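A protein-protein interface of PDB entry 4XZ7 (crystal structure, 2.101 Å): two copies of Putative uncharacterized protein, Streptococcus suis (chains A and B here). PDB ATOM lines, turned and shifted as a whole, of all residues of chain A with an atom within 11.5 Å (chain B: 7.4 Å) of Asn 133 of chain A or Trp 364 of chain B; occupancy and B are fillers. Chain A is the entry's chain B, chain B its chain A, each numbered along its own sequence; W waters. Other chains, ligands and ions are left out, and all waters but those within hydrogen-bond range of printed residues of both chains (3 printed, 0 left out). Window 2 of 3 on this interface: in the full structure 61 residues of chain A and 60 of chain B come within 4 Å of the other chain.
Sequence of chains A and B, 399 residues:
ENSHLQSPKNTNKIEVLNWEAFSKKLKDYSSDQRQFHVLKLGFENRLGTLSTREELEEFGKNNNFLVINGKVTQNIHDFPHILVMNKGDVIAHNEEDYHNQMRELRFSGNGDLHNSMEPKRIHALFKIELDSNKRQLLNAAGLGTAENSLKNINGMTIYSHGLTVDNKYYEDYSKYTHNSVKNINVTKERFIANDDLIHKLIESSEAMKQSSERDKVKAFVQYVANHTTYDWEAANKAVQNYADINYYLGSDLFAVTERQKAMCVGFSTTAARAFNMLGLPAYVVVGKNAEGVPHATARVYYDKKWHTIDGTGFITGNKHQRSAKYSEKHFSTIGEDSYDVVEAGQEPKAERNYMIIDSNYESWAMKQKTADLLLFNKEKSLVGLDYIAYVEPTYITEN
Asn 133 of chain A touches Tyr 361 of chain B (OD1 to CD1, 3.3 Å). ND2 of Asn 133 of chain A touches CD2 of Trp 364 of chain B, 3.5 Å away. Leu 375 of chain B touches Lys 134 of chain A (CD1 to O, 3.99 Å). CB of Gln 136 of chain A touches CE1 of Tyr 361 of chain B (3.6 Å). Tyr 361 of chain B touches Leu 137 of chain A (OH to CD2, 3.0 Å). Trp 364 of chain B touches Leu 137 of chain A (CH2 to CD1, 3.8 Å). CD2 of Leu 137 of chain A touches O of Leu 373 of chain B, 3.2 Å away. Leu 375 of chain B touches Leu 137 of chain A (CD1 to CB, 3.6 Å). CD1 of Leu 375 of chain B touches CD2 of Leu 138 of chain A (3.7 Å).
No position is printed for both chains. Of the 9 pairs that touch across the chains among the printed residues, none has its exchanged pair printed and touching as well.
The side-chain carboxylate (OD1) of Asp 358 of chain B lies within hydrogen-bond range of the backbone NH (N) of Tyr 361 of chain B, at 3.0 Å. NE1 of Trp 364 of chain B lies close to NE2 of Gln 368 of chain B, 3.0 Å away. N of Asn 133 of chain A lies close to OD1 of Asp 131 of chain A, at 3.5 Å. N of Lys 134 of chain A sits at hydrogen-bond distance from OD1 of Asp 131 of chain A (3.0 Å). O of Leu 138 of chain A lies within hydrogen-bond range of N of Leu 143 of chain A (2.9 Å).
Of chain B, only Tyr 361 (3.3 Å) and Trp 364 (3.5 Å) come within 4 Å of Asn 133 of chain A. Of chain A, only Asn 133 and Leu 137 come within 4 Å of Trp 364 of chain B. No residue of chain B comes within 4 Å of Ser 132 of chain A. Tyr 361 of chain B touches three residues of chain A. No residue of chain A comes within 4 Å of Ser 363 of chain B. No residue of chain A comes within 4 Å of Ala 365 of chain B. Met 366 of chain B touches none of the printed residues of chain A. No residue of chain A comes within 4 Å of Lys 367 of chain B. No residue of chain A comes within 4 Å of Gln 368 of chain B. Leu 373 of chain B touches one residue of chain A. Printed residues of chain A within 4 Å of Leu 375 of chain B: Lys 134 (3.99 Å), Leu 137 (3.6 Å) and Leu 138 (3.7 Å). Printed residues of chain B within 4 Å of Gln 136 of chain A: Tyr 361 (3.6 Å). Of the printed residues of chain B, Leu 137 of chain A touches Tyr 361 (3.0 Å), Trp 364 (3.8 Å), Leu 373 (3.2 Å) and Leu 375 (3.6 Å). Asp 131 of chain A touches none of the printed residues of chain B. Gly 144 of chain A touches none of the printed residues of chain B. The nearest residue of chain A that does not touch Trp 364 of chain B is Lys 134 of chain A (5.4 Å). The nearest printed residue of chain B that does not touch Leu 137 of chain A is Asp 372 of chain B (4.1 Å).
Along chain B the printed residues that touch a printed residue of chain A span positions 361 to 375. Among the printed residues, 9 pairs touch across the chains. Among the printed residues, no Asp or Glu carboxylate lies within 4 Å of a Lys or Arg side-chain nitrogen of the other chain.
Water W2 lies within hydrogen-bond range of OD2 of Asp 358 of chain B and OE1 of Gln 136 of chain A. Water W1 bridges the backbone carbonyl oxygen (O) of Leu 375 of chain B (2.8 Å) and the backbone NH (N) of Leu 105 of chain A (2.9 Å). Water W3 lies within hydrogen-bond range of the backbone carbonyl oxygen (O) of Leu 137 of chain A (2.8 Å) and the backbone carbonyl oxygen (O) of Leu 373 of chain B (2.9 Å).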
ATOM      1  N   LEU A 105     -18.887  17.732   6.988  1.00  0.00           N
ATOM      2  CA  LEU A 105     -18.833  19.148   6.651  1.00  0.00           C
ATOM      3  C   LEU A 105     -20.251  19.673   6.472  1.00  0.00           C
ATOM      4  O   LEU A 105     -21.084  19.018   5.848  1.00  0.00           O
ATOM      5  CB  LEU A 105     -18.036  19.387   5.373  1.00  0.00           C
ATOM      6  CG  LEU A 105     -16.546  19.082   5.301  1.00  0.00           C
ATOM      7  CD1 LEU A 105     -16.037  19.690   4.004  1.00  0.00           C
ATOM      8  CD2 LEU A 105     -15.791  19.660   6.489  1.00  0.00           C
ATOM      9  N   GLU A 129     -11.543  23.271  18.741  1.00  0.00           N
ATOM     10  CA  GLU A 129     -10.907  24.042  17.676  1.00  0.00           C
ATOM     11  C   GLU A 129     -10.847  23.217  16.392  1.00  0.00           C
ATOM     12  O   GLU A 129     -11.005  21.995  16.414  1.00  0.00           O
ATOM     13  CB  GLU A 129      -9.508  24.495  18.090  1.00  0.00           C
ATOM     14  CG  GLU A 129      -8.712  23.471  18.872  1.00  0.00           C
ATOM     15  CD  GLU A 129      -7.237  23.825  18.969  1.00  0.00           C
ATOM     16  OE1 GLU A 129      -6.424  23.046  18.426  1.00  0.00           O
ATOM     17  OE2 GLU A 129      -6.887  24.872  19.578  1.00  0.00           O
ATOM     18  N   LEU A 130     -10.646  23.890  15.268  1.00  0.00           N
ATOM     19  CA  LEU A 130     -10.294  23.192  14.029  1.00  0.00           C
ATOM     20  C   LEU A 130      -8.817  23.451  13.752  1.00  0.00           C
ATOM     21  O   LEU A 130      -8.405  24.615  13.641  1.00  0.00           O
ATOM     22  CB  LEU A 130     -11.162  23.664  12.859  1.00  0.00           C
ATOM     23  CG  LEU A 130     -12.660  23.433  13.042  1.00  0.00           C
ATOM     24  CD1 LEU A 130     -13.441  24.021  11.871  1.00  0.00           C
ATOM     25  CD2 LEU A 130     -12.956  21.943  13.206  1.00  0.00           C
ATOM     26  N   ASP A 131      -8.005  22.396  13.670  1.00  0.00           N
ATOM     27  CA  ASP A 131      -6.561  22.612  13.629  1.00  0.00           C
ATOM     28  C   ASP A 131      -6.066  23.031  12.239  1.00  0.00           C
ATOM     29  O   ASP A 131      -6.824  23.059  11.265  1.00  0.00           O
ATOM     30  CB  ASP A 131      -5.797  21.372  14.138  1.00  0.00           C
ATOM     31  CG  ASP A 131      -6.033  20.127  13.307  1.00  0.00           C
ATOM     32  OD1 ASP A 131      -6.599  20.218  12.189  1.00  0.00           O
ATOM     33  OD2 ASP A 131      -5.632  19.039  13.791  1.00  0.00           O
ATOM     34  N   SER A 132      -4.793  23.396  12.167  1.00  0.00           N
ATOM     35  CA  SER A 132      -4.214  23.919  10.940  1.00  0.00           C
ATOM     36  C   SER A 132      -4.219  22.875   9.815  1.00  0.00           C
ATOM     37  O   SER A 132      -4.280  23.234   8.642  1.00  0.00           O
ATOM     38  CB  SER A 132      -2.790  24.404  11.211  1.00  0.00           C
ATOM     39  OG  SER A 132      -2.037  23.356  11.803  1.00  0.00           O
ATOM     40  N   ASN A 133      -4.167  21.586  10.157  1.00  0.00           N
ATOM     41  CA  ASN A 133      -4.194  20.535   9.125  1.00  0.00           C
ATOM     42  C   ASN A 133      -5.548  20.509   8.411  1.00  0.00           C
ATOM     43  O   ASN A 133      -5.624  20.434   7.165  1.00  0.00           O
ATOM     44  CB  ASN A 133      -3.904  19.145   9.715  1.00  0.00           C
ATOM     45  CG  ASN A 133      -2.448  18.974  10.177  1.00  0.00           C
ATOM     46  OD1 ASN A 133      -1.547  19.681   9.725  1.00  0.00           O
ATOM     47  ND2 ASN A 133      -2.222  18.018  11.088  1.00  0.00           N
ATOM     48  N   LYS A 134      -6.616  20.553   9.201  1.00  0.00           N
ATOM     49  CA  LYS A 134      -7.956  20.518   8.636  1.00  0.00           C
ATOM     50  C   LYS A 134      -8.206  21.789   7.827  1.00  0.00           C
ATOM     51  O   LYS A 134      -8.816  21.741   6.763  1.00  0.00           O
ATOM     52  CB  LYS A 134      -9.044  20.355   9.719  1.00  0.00           C
ATOM     53  CG  LYS A 134     -10.441  20.326   9.088  1.00  0.00           C
ATOM     54  CD  LYS A 134     -11.584  19.959  10.012  1.00  0.00           C
ATOM     55  CE  LYS A 134     -12.880  19.844   9.187  1.00  0.00           C
ATOM     56  NZ  LYS A 134     -14.182  19.779   9.949  1.00  0.00           N
ATOM     57  N   ARG A 135      -7.749  22.924   8.332  1.00  0.00           N
ATOM     58  CA  ARG A 135      -7.932  24.179   7.601  1.00  0.00           C
ATOM     59  C   ARG A 135      -7.122  24.184   6.294  1.00  0.00           C
ATOM     60  O   ARG A 135      -7.543  24.745   5.290  1.00  0.00           O
ATOM     61  CB  ARG A 135      -7.555  25.361   8.486  1.00  0.00           C
ATOM     62  CG  ARG A 135      -8.529  25.527   9.644  1.00  0.00           C
ATOM     63  CD  ARG A 135      -8.097  26.609  10.633  1.00  0.00           C
ATOM     64  NE  ARG A 135      -9.103  26.755  11.684  1.00  0.00           N
ATOM     65  CZ  ARG A 135     -10.251  27.416  11.537  1.00  0.00           C
ATOM     66  NH1 ARG A 135     -10.555  28.000  10.376  1.00  0.00           N
ATOM     67  NH2 ARG A 135     -11.105  27.483  12.550  1.00  0.00           N
ATOM     68  N   GLN A 136      -5.961  23.537   6.308  1.00  0.00           N
ATOM     69  CA  GLN A 136      -5.164  23.420   5.104  1.00  0.00           C
ATOM     70  C   GLN A 136      -5.922  22.575   4.065  1.00  0.00           C
ATOM     71  O   GLN A 136      -5.933  22.915   2.876  1.00  0.00           O
ATOM     72  CB  GLN A 136      -3.798  22.807   5.421  1.00  0.00           C
ATOM     73  CG  GLN A 136      -2.766  22.991   4.333  1.00  0.00           C
ATOM     74  CD  GLN A 136      -2.311  24.426   4.192  1.00  0.00           C
ATOM     75  OE1 GLN A 136      -1.519  24.923   5.007  1.00  0.00           O
ATOM     76  NE2 GLN A 136      -2.777  25.097   3.149  1.00  0.00           N
ATOM     77  N   LEU A 137      -6.564  21.497   4.512  1.00  0.00           N
ATOM     78  CA  LEU A 137      -7.333  20.673   3.589  1.00  0.00           C
ATOM     79  C   LEU A 137      -8.579  21.415   3.049  1.00  0.00           C
ATOM     80  O   LEU A 137      -8.962  21.261   1.870  1.00  0.00           O
ATOM     81  CB  LEU A 137      -7.738  19.361   4.269  1.00  0.00           C
ATOM     82  CG  LEU A 137      -6.595  18.374   4.511  1.00  0.00           C
ATOM     83  CD1 LEU A 137      -7.063  17.232   5.417  1.00  0.00           C
ATOM     84  CD2 LEU A 137      -6.100  17.820   3.181  1.00  0.00           C
ATOM     85  N   LEU A 138      -9.203  22.220   3.908  1.00  0.00           N
ATOM     86  CA  LEU A 138     -10.346  23.018   3.464  1.00  0.00           C
ATOM     87  C   LEU A 138      -9.880  23.956   2.357  1.00  0.00           C
ATOM     88  O   LEU A 138     -10.499  24.020   1.281  1.00  0.00           O
ATOM     89  CB  LEU A 138     -10.966  23.807   4.618  1.00  0.00           C
ATOM     90  CG  LEU A 138     -11.845  23.021   5.587  1.00  0.00           C
ATOM     91  CD1 LEU A 138     -12.176  23.888   6.794  1.00  0.00           C
ATOM     92  CD2 LEU A 138     -13.141  22.505   4.924  1.00  0.00           C
ATOM     93  N   ASN A 139      -8.771  24.648   2.620  1.00  0.00           N
ATOM     94  CA  ASN A 139      -8.163  25.537   1.625  1.00  0.00           C
ATOM     95  C   ASN A 139      -7.846  24.798   0.326  1.00  0.00           C
ATOM     96  O   ASN A 139      -7.963  25.356  -0.770  1.00  0.00           O
ATOM     97  CB  ASN A 139      -6.880  26.178   2.172  1.00  0.00           C
ATOM     98  CG  ASN A 139      -6.330  27.252   1.245  1.00  0.00           C
ATOM     99  OD1 ASN A 139      -6.940  28.299   1.060  1.00  0.00           O
ATOM    100  ND2 ASN A 139      -5.178  26.994   0.664  1.00  0.00           N
ATOM    101  N   ALA A 140      -7.431  23.541   0.467  1.00  0.00           N
ATOM    102  CA  ALA A 140      -7.115  22.697  -0.671  1.00  0.00           C
ATOM    103  C   ALA A 140      -8.371  22.312  -1.440  1.00  0.00           C
ATOM    104  O   ALA A 140      -8.277  21.811  -2.552  1.00  0.00           O
ATOM    105  CB  ALA A 140      -6.369  21.426  -0.217  1.00  0.00           C
ATOM    106  N   ALA A 141      -9.544  22.491  -0.836  1.00  0.00           N
ATOM    107  CA  ALA A 141     -10.792  22.319  -1.595  1.00  0.00           C
ATOM    108  C   ALA A 141     -11.422  23.662  -1.950  1.00  0.00           C
ATOM    109  O   ALA A 141     -12.549  23.720  -2.438  1.00  0.00           O
ATOM    110  CB  ALA A 141     -11.792  21.461  -0.811  1.00  0.00           C
ATOM    111  N   GLY A 142     -10.697  24.746  -1.683  1.00  0.00           N
ATOM    112  CA  GLY A 142     -11.203  26.083  -1.966  1.00  0.00           C
ATOM    113  C   GLY A 142     -12.203  26.630  -0.964  1.00  0.00           C
ATOM    114  O   GLY A 142     -12.893  27.621  -1.233  1.00  0.00           O
ATOM    115  N   LEU A 143     -12.267  25.996   0.205  1.00  0.00           N
ATOM    116  CA  LEU A 143     -13.239  26.362   1.231  1.00  0.00           C
ATOM    117  C   LEU A 143     -12.575  27.078   2.398  1.00  0.00           C
ATOM    118  O   LEU A 143     -11.362  26.962   2.601  1.00  0.00           O
ATOM    119  CB  LEU A 143     -13.961  25.124   1.754  1.00  0.00           C
ATOM    120  CG  LEU A 143     -14.683  24.235   0.741  1.00  0.00           C
ATOM    121  CD1 LEU A 143     -15.088  22.880   1.363  1.00  0.00           C
ATOM    122  CD2 LEU A 143     -15.916  24.966   0.167  1.00  0.00           C
ATOM    123  N   GLY A 144     -13.383  27.803   3.167  1.00  0.00           N
ATOM    124  CA  GLY A 144     -12.959  28.401   4.425  1.00  0.00           C
ATOM    125  C   GLY A 144     -14.046  28.237   5.467  1.00  0.00           C
ATOM    126  O   GLY A 144     -15.155  27.783   5.168  1.00  0.00           O
ATOM    127  N   THR A 145     -13.739  28.615   6.705  1.00  0.00           N
ATOM    128  CA  THR A 145     -14.661  28.425   7.826  1.00  0.00           C
ATOM    129  C   THR A 145     -14.114  29.292   8.938  1.00  0.00           C
ATOM    130  O   THR A 145     -12.907  29.530   8.996  1.00  0.00           O
ATOM    131  CB  THR A 145     -14.769  26.944   8.272  1.00  0.00           C
ATOM    132  OG1 THR A 145     -16.001  26.725   8.963  1.00  0.00           O
ATOM    133  CG2 THR A 145     -13.632  26.586   9.203  1.00  0.00           C
ATOM    134  N   GLU A 147     -12.566  31.195  12.035  1.00  0.00           N
ATOM    135  CA  GLU A 147     -11.346  30.864  12.752  1.00  0.00           C
ATOM    136  C   GLU A 147     -11.620  30.469  14.188  1.00  0.00           C
ATOM    137  O   GLU A 147     -12.714  30.717  14.712  1.00  0.00           O
ATOM    138  CB  GLU A 147     -10.399  32.058  12.705  1.00  0.00           C
ATOM    139  CG  GLU A 147     -10.211  32.585  11.276  1.00  0.00           C
ATOM    140  CD  GLU A 147      -9.591  31.554  10.323  1.00  0.00           C
ATOM    141  OE1 GLU A 147     -10.146  31.367   9.210  1.00  0.00           O
ATOM    142  OE2 GLU A 147      -8.547  30.946  10.685  1.00  0.00           O
ATOM    143  N   ASN A 148     -10.616  29.860  14.815  1.00  0.00           N
ATOM    144  CA  ASN A 148     -10.694  29.488  16.221  1.00  0.00           C
ATOM    145  C   ASN A 148     -10.655  30.719  17.096  1.00  0.00           C
ATOM    146  O   ASN A 148      -9.885  31.628  16.836  1.00  0.00           O
ATOM    147  CB  ASN A 148      -9.527  28.573  16.601  1.00  0.00           C
ATOM    148  CG  ASN A 148      -9.514  27.285  15.810  1.00  0.00           C
ATOM    149  OD1 ASN A 148     -10.580  26.736  15.467  1.00  0.00           O
ATOM    150  ND2 ASN A 148      -8.311  26.782  15.519  1.00  0.00           N
ATOM    151  N   TRP B 306       7.883  15.553  -1.823  1.00  0.00           N
ATOM    152  CA  TRP B 306       6.962  16.638  -2.078  1.00  0.00           C
ATOM    153  C   TRP B 306       7.477  17.491  -3.228  1.00  0.00           C
ATOM    154  O   TRP B 306       8.667  17.762  -3.318  1.00  0.00           O
ATOM    155  CB  TRP B 306       6.751  17.471  -0.815  1.00  0.00           C
ATOM    156  CG  TRP B 306       5.770  16.818   0.120  1.00  0.00           C
ATOM    157  CD1 TRP B 306       6.046  15.960   1.156  1.00  0.00           C
ATOM    158  CD2 TRP B 306       4.351  16.941   0.072  1.00  0.00           C
ATOM    159  NE1 TRP B 306       4.872  15.568   1.773  1.00  0.00           N
ATOM    160  CE2 TRP B 306       3.819  16.150   1.114  1.00  0.00           C
ATOM    161  CE3 TRP B 306       3.471  17.659  -0.748  1.00  0.00           C
ATOM    162  CZ2 TRP B 306       2.454  16.069   1.365  1.00  0.00           C
ATOM    163  CZ3 TRP B 306       2.118  17.569  -0.509  1.00  0.00           C
ATOM    164  CH2 TRP B 306       1.616  16.774   0.541  1.00  0.00           C
ATOM    165  N   ASP B 358       4.624  24.301   4.112  1.00  0.00           N
ATOM    166  CA  ASP B 358       4.501  23.865   5.494  1.00  0.00           C
ATOM    167  C   ASP B 358       4.974  22.426   5.600  1.00  0.00           C
ATOM    168  O   ASP B 358       4.208  21.490   5.372  1.00  0.00           O
ATOM    169  CB  ASP B 358       3.060  24.014   5.994  1.00  0.00           C
ATOM    170  CG  ASP B 358       2.935  23.737   7.501  1.00  0.00           C
ATOM    171  OD1 ASP B 358       3.791  23.014   8.053  1.00  0.00           O
ATOM    172  OD2 ASP B 358       1.985  24.238   8.136  1.00  0.00           O
ATOM    173  N   SER B 359       6.244  22.274   5.962  1.00  0.00           N
ATOM    174  CA  SER B 359       6.926  20.984   6.026  1.00  0.00           C
ATOM    175  C   SER B 359       6.299  20.021   7.016  1.00  0.00           C
ATOM    176  O   SER B 359       6.233  18.812   6.769  1.00  0.00           O
ATOM    177  CB  SER B 359       8.400  21.187   6.391  1.00  0.00           C
ATOM    178  OG  SER B 359       9.190  21.448   5.236  1.00  0.00           O
ATOM    179  N   ASN B 360       5.849  20.552   8.146  1.00  0.00           N
ATOM    180  CA  ASN B 360       5.186  19.721   9.138  1.00  0.00           C
ATOM    181  C   ASN B 360       3.862  19.218   8.559  1.00  0.00           C
ATOM    182  O   ASN B 360       3.471  18.050   8.754  1.00  0.00           O
ATOM    183  CB  ASN B 360       4.975  20.502  10.445  1.00  0.00           C
ATOM    184  CG  ASN B 360       6.275  20.670  11.245  1.00  0.00           C
ATOM    185  OD1 ASN B 360       7.182  19.844  11.153  1.00  0.00           O
ATOM    186  ND2 ASN B 360       6.360  21.738  12.029  1.00  0.00           N
ATOM    187  N   TYR B 361       3.179  20.088   7.820  1.00  0.00           N
ATOM    188  CA  TYR B 361       1.922  19.674   7.198  1.00  0.00           C
ATOM    189  C   TYR B 361       2.203  18.587   6.154  1.00  0.00           C
ATOM    190  O   TYR B 361       1.501  17.579   6.093  1.00  0.00           O
ATOM    191  CB  TYR B 361       1.165  20.843   6.539  1.00  0.00           C
ATOM    192  CG  TYR B 361      -0.040  20.303   5.798  1.00  0.00           C
ATOM    193  CD1 TYR B 361      -1.233  20.049   6.471  1.00  0.00           C
ATOM    194  CD2 TYR B 361       0.046  19.954   4.446  1.00  0.00           C
ATOM    195  CE1 TYR B 361      -2.322  19.503   5.807  1.00  0.00           C
ATOM    196  CE2 TYR B 361      -1.028  19.398   3.779  1.00  0.00           C
ATOM    197  CZ  TYR B 361      -2.203  19.176   4.465  1.00  0.00           C
ATOM    198  OH  TYR B 361      -3.266  18.620   3.813  1.00  0.00           O
ATOM    199  N   GLU B 362       3.219  18.802   5.329  1.00  0.00           N
ATOM    200  CA  GLU B 362       3.607  17.807   4.334  1.00  0.00           C
ATOM    201  C   GLU B 362       3.904  16.458   4.959  1.00  0.00           C
ATOM    202  O   GLU B 362       3.455  15.426   4.452  1.00  0.00           O
ATOM    203  CB  GLU B 362       4.805  18.317   3.519  1.00  0.00           C
ATOM    204  CG  GLU B 362       4.315  19.412   2.581  1.00  0.00           C
ATOM    205  CD  GLU B 362       5.392  20.104   1.783  1.00  0.00           C
ATOM    206  OE1 GLU B 362       6.518  19.581   1.622  1.00  0.00           O
ATOM    207  OE2 GLU B 362       5.076  21.193   1.296  1.00  0.00           O
ATOM    208  N   SER B 363       4.617  16.457   6.081  1.00  0.00           N
ATOM    209  CA  SER B 363       4.915  15.190   6.746  1.00  0.00           C
ATOM    210  C   SER B 363       3.659  14.499   7.228  1.00  0.00           C
ATOM    211  O   SER B 363       3.563  13.264   7.156  1.00  0.00           O
ATOM    212  CB  SER B 363       5.865  15.396   7.934  1.00  0.00           C
ATOM    213  OG  SER B 363       7.109  15.895   7.489  1.00  0.00           O
ATOM    214  N   TRP B 364       2.721  15.281   7.770  1.00  0.00           N
ATOM    215  CA  TRP B 364       1.454  14.709   8.228  1.00  0.00           C
ATOM    216  C   TRP B 364       0.576  14.178   7.085  1.00  0.00           C
ATOM    217  O   TRP B 364       0.070  13.048   7.154  1.00  0.00           O
ATOM    218  CB  TRP B 364       0.656  15.741   9.026  1.00  0.00           C
ATOM    219  CG  TRP B 364      -0.741  15.266   9.392  1.00  0.00           C
ATOM    220  CD1 TRP B 364      -1.096  14.488  10.464  1.00  0.00           C
ATOM    221  CD2 TRP B 364      -1.963  15.548   8.681  1.00  0.00           C
ATOM    222  NE1 TRP B 364      -2.463  14.264  10.460  1.00  0.00           N
ATOM    223  CE2 TRP B 364      -3.015  14.916   9.382  1.00  0.00           C
ATOM    224  CE3 TRP B 364      -2.270  16.284   7.525  1.00  0.00           C
ATOM    225  CZ2 TRP B 364      -4.349  14.980   8.953  1.00  0.00           C
ATOM    226  CZ3 TRP B 364      -3.596  16.347   7.104  1.00  0.00           C
ATOM    227  CH2 TRP B 364      -4.613  15.703   7.817  1.00  0.00           C
ATOM    228  N   ALA B 365       0.389  14.985   6.043  1.00  0.00           N
ATOM    229  CA  ALA B 365      -0.568  14.639   4.981  1.00  0.00           C
ATOM    230  C   ALA B 365      -0.170  13.410   4.165  1.00  0.00           C
ATOM    231  O   ALA B 365      -1.034  12.617   3.759  1.00  0.00           O
ATOM    232  CB  ALA B 365      -0.782  15.842   4.039  1.00  0.00           C
ATOM    233  N   MET B 366       1.129  13.247   3.926  1.00  0.00           N
ATOM    234  CA  MET B 366       1.622  12.129   3.118  1.00  0.00           C
ATOM    235  C   MET B 366       1.365  10.763   3.754  1.00  0.00           C
ATOM    236  O   MET B 366       1.389   9.757   3.057  1.00  0.00           O
ATOM    237  CB  MET B 366       3.124  12.281   2.823  1.00  0.00           C
ATOM    238  CG  MET B 366       4.043  12.052   4.023  1.00  0.00           C
ATOM    239  SD  MET B 366       5.784  12.299   3.631  1.00  0.00           S
ATOM    240  CE  MET B 366       6.545  11.967   5.221  1.00  0.00           C
ATOM    241  N   LYS B 367       1.097  10.737   5.061  1.00  0.00           N
ATOM    242  CA  LYS B 367       0.851   9.471   5.773  1.00  0.00           C
ATOM    243  C   LYS B 367      -0.643   9.174   5.963  1.00  0.00           C
ATOM    244  O   LYS B 367      -1.011   8.125   6.490  1.00  0.00           O
ATOM    245  CB  LYS B 367       1.538   9.480   7.150  1.00  0.00           C
ATOM    246  CG  LYS B 367       3.056   9.613   7.125  1.00  0.00           C
ATOM    247  CD  LYS B 367       3.640   9.301   8.507  1.00  0.00           C
ATOM    248  CE  LYS B 367       5.073   9.800   8.662  1.00  0.00           C
ATOM    249  NZ  LYS B 367       5.095  11.283   8.802  1.00  0.00           N
ATOM    250  N   GLN B 368      -1.498  10.100   5.544  1.00  0.00           N
ATOM    251  CA  GLN B 368      -2.952   9.946   5.693  1.00  0.00           C
ATOM    252  C   GLN B 368      -3.567   9.042   4.623  1.00  0.00           C
ATOM    253  O   GLN B 368      -3.022   8.899   3.522  1.00  0.00           O
ATOM    254  CB  GLN B 368      -3.631  11.322   5.639  1.00  0.00           C
ATOM    255  CG  GLN B 368      -3.142  12.319   6.701  1.00  0.00           C
ATOM    256  CD  GLN B 368      -3.282  11.789   8.132  1.00  0.00           C
ATOM    257  OE1 GLN B 368      -4.376  11.447   8.576  1.00  0.00           O
ATOM    258  NE2 GLN B 368      -2.166  11.726   8.853  1.00  0.00           N
ATOM    259  N   LYS B 369      -4.710   8.435   4.927  1.00  0.00           N
ATOM    260  CA  LYS B 369      -5.486   7.811   3.872  1.00  0.00           C
ATOM    261  C   LYS B 369      -5.915   8.961   2.966  1.00  0.00           C
ATOM    262  O   LYS B 369      -6.446   9.963   3.446  1.00  0.00           O
ATOM    263  CB  LYS B 369      -6.687   7.037   4.422  1.00  0.00           C
ATOM    264  CG  LYS B 369      -6.339   5.761   5.185  1.00  0.00           C
ATOM    265  CD  LYS B 369      -7.609   5.086   5.689  1.00  0.00           C
ATOM    266  CE  LYS B 369      -7.488   4.631   7.138  1.00  0.00           C
ATOM    267  NZ  LYS B 369      -8.837   4.387   7.730  1.00  0.00           N
ATOM    268  N   ASP B 372      -9.262  10.659   3.191  1.00  0.00           N
ATOM    269  CA  ASP B 372      -9.438  11.555   4.329  1.00  0.00           C
ATOM    270  C   ASP B 372      -8.959  12.969   4.010  1.00  0.00           C
ATOM    271  O   ASP B 372      -9.374  13.922   4.663  1.00  0.00           O
ATOM    272  CB  ASP B 372      -8.703  11.038   5.558  1.00  0.00           C
ATOM    273  CG  ASP B 372      -9.349   9.786   6.137  1.00  0.00           C
ATOM    274  OD1 ASP B 372     -10.532   9.522   5.817  1.00  0.00           O
ATOM    275  OD2 ASP B 372      -8.672   9.071   6.902  1.00  0.00           O
ATOM    276  N   LEU B 373      -8.078  13.106   3.027  1.00  0.00           N
ATOM    277  CA  LEU B 373      -7.599  14.430   2.651  1.00  0.00           C
ATOM    278  C   LEU B 373      -8.728  15.213   1.970  1.00  0.00           C
ATOM    279  O   LEU B 373      -8.658  16.434   1.879  1.00  0.00           O
ATOM    280  CB  LEU B 373      -6.369  14.331   1.740  1.00  0.00           C
ATOM    281  CG  LEU B 373      -5.144  13.646   2.367  1.00  0.00           C
ATOM    282  CD1 LEU B 373      -3.975  13.536   1.381  1.00  0.00           C
ATOM    283  CD2 LEU B 373      -4.719  14.375   3.661  1.00  0.00           C
ATOM    284  N   LEU B 375     -11.899  15.289   2.954  1.00  0.00           N
ATOM    285  CA  LEU B 375     -12.800  15.764   4.013  1.00  0.00           C
ATOM    286  C   LEU B 375     -14.284  15.456   3.767  1.00  0.00           C
ATOM    287  O   LEU B 375     -15.041  15.264   4.705  1.00  0.00           O
ATOM    288  CB  LEU B 375     -12.636  17.275   4.221  1.00  0.00           C
ATOM    289  CG  LEU B 375     -11.276  17.796   4.678  1.00  0.00           C
ATOM    290  CD1 LEU B 375     -11.324  19.327   4.814  1.00  0.00           C
ATOM    291  CD2 LEU B 375     -10.869  17.116   6.008  1.00  0.00           C
HETATM  292  O   HOH W   1     -17.589  15.361   5.814  1.00  0.00           O
HETATM  293  O   HOH W   2      -0.407  23.918   7.787  1.00  0.00           O
HETATM  294  O   HOH W   3      -9.485  18.863   0.530  1.00  0.00           O
